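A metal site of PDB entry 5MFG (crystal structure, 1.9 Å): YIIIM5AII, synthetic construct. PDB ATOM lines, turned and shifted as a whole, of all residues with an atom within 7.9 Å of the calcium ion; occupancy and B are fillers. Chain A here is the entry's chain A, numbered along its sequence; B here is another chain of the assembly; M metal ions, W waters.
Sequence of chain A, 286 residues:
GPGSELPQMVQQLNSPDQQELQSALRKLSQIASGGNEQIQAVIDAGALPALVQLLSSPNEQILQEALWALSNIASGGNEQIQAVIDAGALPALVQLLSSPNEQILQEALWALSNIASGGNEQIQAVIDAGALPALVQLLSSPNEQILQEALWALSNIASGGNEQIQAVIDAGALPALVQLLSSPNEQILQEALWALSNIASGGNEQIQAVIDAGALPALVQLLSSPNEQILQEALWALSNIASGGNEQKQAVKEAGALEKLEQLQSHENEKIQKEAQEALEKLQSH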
ATOM      1  N   SER A  99      31.628  17.338  16.111  1.00  0.00           N
ATOM      2  CA  SER A  99      31.082  16.235  16.895  1.00  0.00           C
ATOM      3  C   SER A  99      29.570  16.394  17.046  1.00  0.00           C
ATOM      4  O   SER A  99      29.081  17.515  17.235  1.00  0.00           O
ATOM      5  CB  SER A  99      31.731  16.194  18.275  1.00  0.00           C
ATOM      6  OG  SER A  99      31.053  15.281  19.119  1.00  0.00           O
ATOM      7  N   PRO A 100      28.806  15.304  16.976  1.00  0.00           N
ATOM      8  CA  PRO A 100      27.379  15.372  17.320  1.00  0.00           C
ATOM      9  C   PRO A 100      27.125  15.333  18.818  1.00  0.00           C
ATOM     10  O   PRO A 100      25.957  15.373  19.232  1.00  0.00           O
ATOM     11  CB  PRO A 100      26.803  14.128  16.633  1.00  0.00           C
ATOM     12  CG  PRO A 100      27.918  13.161  16.654  1.00  0.00           C
ATOM     13  CD  PRO A 100      29.192  13.962  16.502  1.00  0.00           C
ATOM     14  N   ASN A 101      28.175  15.246  19.633  1.00  0.00           N
ATOM     15  CA  ASN A 101      28.048  15.139  21.083  1.00  0.00           C
ATOM     16  C   ASN A 101      28.128  16.556  21.659  1.00  0.00           C
ATOM     17  O   ASN A 101      29.197  17.137  21.743  1.00  0.00           O
ATOM     18  CB  ASN A 101      29.148  14.243  21.645  1.00  0.00           C
ATOM     19  CG  ASN A 101      29.066  14.099  23.145  1.00  0.00           C
ATOM     20  OD1 ASN A 101      28.679  15.022  23.849  1.00  0.00           O
ATOM     21  ND2 ASN A 101      29.457  12.937  23.633  1.00  0.00           N
ATOM     22  N   GLU A 102      26.975  17.082  22.072  1.00  0.00           N
ATOM     23  CA  GLU A 102      26.925  18.450  22.564  1.00  0.00           C
ATOM     24  C   GLU A 102      27.822  18.649  23.781  1.00  0.00           C
ATOM     25  O   GLU A 102      28.383  19.729  23.973  1.00  0.00           O
ATOM     26  CB  GLU A 102      25.481  18.837  22.899  1.00  0.00           C
ATOM     27  CG  GLU A 102      24.567  18.973  21.688  1.00  0.00           C
ATOM     28  CD  GLU A 102      23.999  17.639  21.211  1.00  0.00           C
ATOM     29  OE1 GLU A 102      24.418  16.590  21.727  1.00  0.00           O
ATOM     30  OE2 GLU A 102      23.138  17.657  20.310  1.00  0.00           O
ATOM     31  N   GLN A 103      27.962  17.623  24.616  1.00  0.00           N
ATOM     32  CA  GLN A 103      28.836  17.728  25.783  1.00  0.00           C
ATOM     33  C   GLN A 103      30.270  17.981  25.355  1.00  0.00           C
ATOM     34  O   GLN A 103      30.925  18.919  25.822  1.00  0.00           O
ATOM     35  CB  GLN A 103      28.732  16.471  26.637  1.00  0.00           C
ATOM     36  CG  GLN A 103      28.632  16.727  28.130  1.00  0.00           C
ATOM     37  CD  GLN A 103      28.382  15.447  28.932  1.00  0.00           C
ATOM     38  OE1 GLN A 103      28.069  14.407  28.372  1.00  0.00           O
ATOM     39  NE2 GLN A 103      28.536  15.548  30.242  1.00  0.00           N
ATOM     40  N   ILE A 146      24.524  25.775  21.877  1.00  0.00           N
ATOM     41  CA  ILE A 146      25.627  25.707  20.921  1.00  0.00           C
ATOM     42  C   ILE A 146      25.888  27.077  20.328  1.00  0.00           C
ATOM     43  O   ILE A 146      27.042  27.475  20.108  1.00  0.00           O
ATOM     44  CB  ILE A 146      25.321  24.665  19.824  1.00  0.00           C
ATOM     45  CG1 ILE A 146      25.270  23.258  20.423  1.00  0.00           C
ATOM     46  CG2 ILE A 146      26.352  24.764  18.720  1.00  0.00           C
ATOM     47  CD1 ILE A 146      24.761  22.207  19.447  1.00  0.00           C
ATOM     48  N   SER B 141      16.873  12.060  25.686  1.00  0.00           N
ATOM     49  CA  SER B 141      17.350  13.091  24.773  1.00  0.00           C
ATOM     50  C   SER B 141      18.591  12.617  24.022  1.00  0.00           C
ATOM     51  O   SER B 141      19.477  11.999  24.615  1.00  0.00           O
ATOM     52  CB  SER B 141      17.669  14.367  25.533  1.00  0.00           C
ATOM     53  OG  SER B 141      18.246  15.331  24.676  1.00  0.00           O
ATOM     54  N   PRO B 142      18.680  12.892  22.711  1.00  0.00           N
ATOM     55  CA  PRO B 142      19.950  12.676  22.006  1.00  0.00           C
ATOM     56  C   PRO B 142      20.994  13.733  22.300  1.00  0.00           C
ATOM     57  O   PRO B 142      22.116  13.633  21.791  1.00  0.00           O
ATOM     58  CB  PRO B 142      19.522  12.733  20.531  1.00  0.00           C
ATOM     59  CG  PRO B 142      18.381  13.666  20.526  1.00  0.00           C
ATOM     60  CD  PRO B 142      17.649  13.429  21.821  1.00  0.00           C
ATOM     61  N   ASN B 143      20.642  14.744  23.081  1.00  0.00           N
ATOM     62  CA  ASN B 143      21.547  15.820  23.446  1.00  0.00           C
ATOM     63  C   ASN B 143      22.261  15.407  24.733  1.00  0.00           C
ATOM     64  O   ASN B 143      21.649  15.401  25.804  1.00  0.00           O
ATOM     65  CB  ASN B 143      20.789  17.127  23.620  1.00  0.00           C
ATOM     66  CG  ASN B 143      21.686  18.279  23.967  1.00  0.00           C
ATOM     67  OD1 ASN B 143      22.672  18.124  24.675  1.00  0.00           O
ATOM     68  ND2 ASN B 143      21.352  19.467  23.465  1.00  0.00           N
ATOM     69  N   GLU B 144      23.539  15.076  24.616  1.00  0.00           N
ATOM     70  CA  GLU B 144      24.305  14.647  25.782  1.00  0.00           C
ATOM     71  C   GLU B 144      24.407  15.753  26.817  1.00  0.00           C
ATOM     72  O   GLU B 144      24.519  15.481  28.014  1.00  0.00           O
ATOM     73  CB  GLU B 144      25.694  14.182  25.360  1.00  0.00           C
ATOM     74  CG  GLU B 144      25.705  12.908  24.526  1.00  0.00           C
ATOM     75  CD  GLU B 144      25.452  13.146  23.047  1.00  0.00           C
ATOM     76  OE1 GLU B 144      24.968  14.242  22.691  1.00  0.00           O
ATOM     77  OE2 GLU B 144      25.743  12.245  22.236  1.00  0.00           O
ATOM     78  N   GLN B 145      24.358  17.010  26.370  1.00  0.00           N
ATOM     79  CA  GLN B 145      24.409  18.137  27.298  1.00  0.00           C
ATOM     80  C   GLN B 145      23.165  18.179  28.172  1.00  0.00           C
ATOM     81  O   GLN B 145      23.258  18.206  29.410  1.00  0.00           O
ATOM     82  CB  GLN B 145      24.553  19.432  26.504  1.00  0.00           C
ATOM     83  CG  GLN B 145      25.384  20.512  27.179  1.00  0.00           C
ATOM     84  CD  GLN B 145      25.677  21.693  26.261  1.00  0.00           C
ATOM     85  OE1 GLN B 145      25.264  21.708  25.097  1.00  0.00           O
ATOM     86  NE2 GLN B 145      26.397  22.672  26.784  1.00  0.00           N
HETATM   87 CA    CA M   1      23.925  14.549  20.518  1.00  0.00          CA
HETATM   88  O   HOH W   1      22.413  15.801  19.332  1.00  0.00           O
HETATM   89  O   HOH W   2      25.024  12.188  19.934  1.00  0.00           O
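The side-chain amide oxygen (OD1) of Asn 143 of chain B is in hydrogen-bond range of the backbone NH (N) of Gln 145 of chain B (2.6 Å). The backbone NH (N) of Asn 143 of chain B sits at hydrogen-bond distance from the side-chain hydroxyl (OG) of Ser 141 of chain B (2.9 Å).
Asn 143 of chain B touches the calcium ion. Within 4 Å of the calcium ion: Pro 100, Glu 102, Pro 142 of chain B, Asn 143 of chain B and Glu 144 of chain B. The nearest printed residue that does not touch the calcium ion is Asn 101 (4.2 Å).
The calcium ion is bound by water W1 (2.3 Å), O of Pro 142 of chain B (2.4 Å), OE1 of Glu 102 (2.4 Å), OE1 of Glu 144 of chain B (2.4 Å), O of Pro 100 (2.5 Å) and water W2 (2.7 Å).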
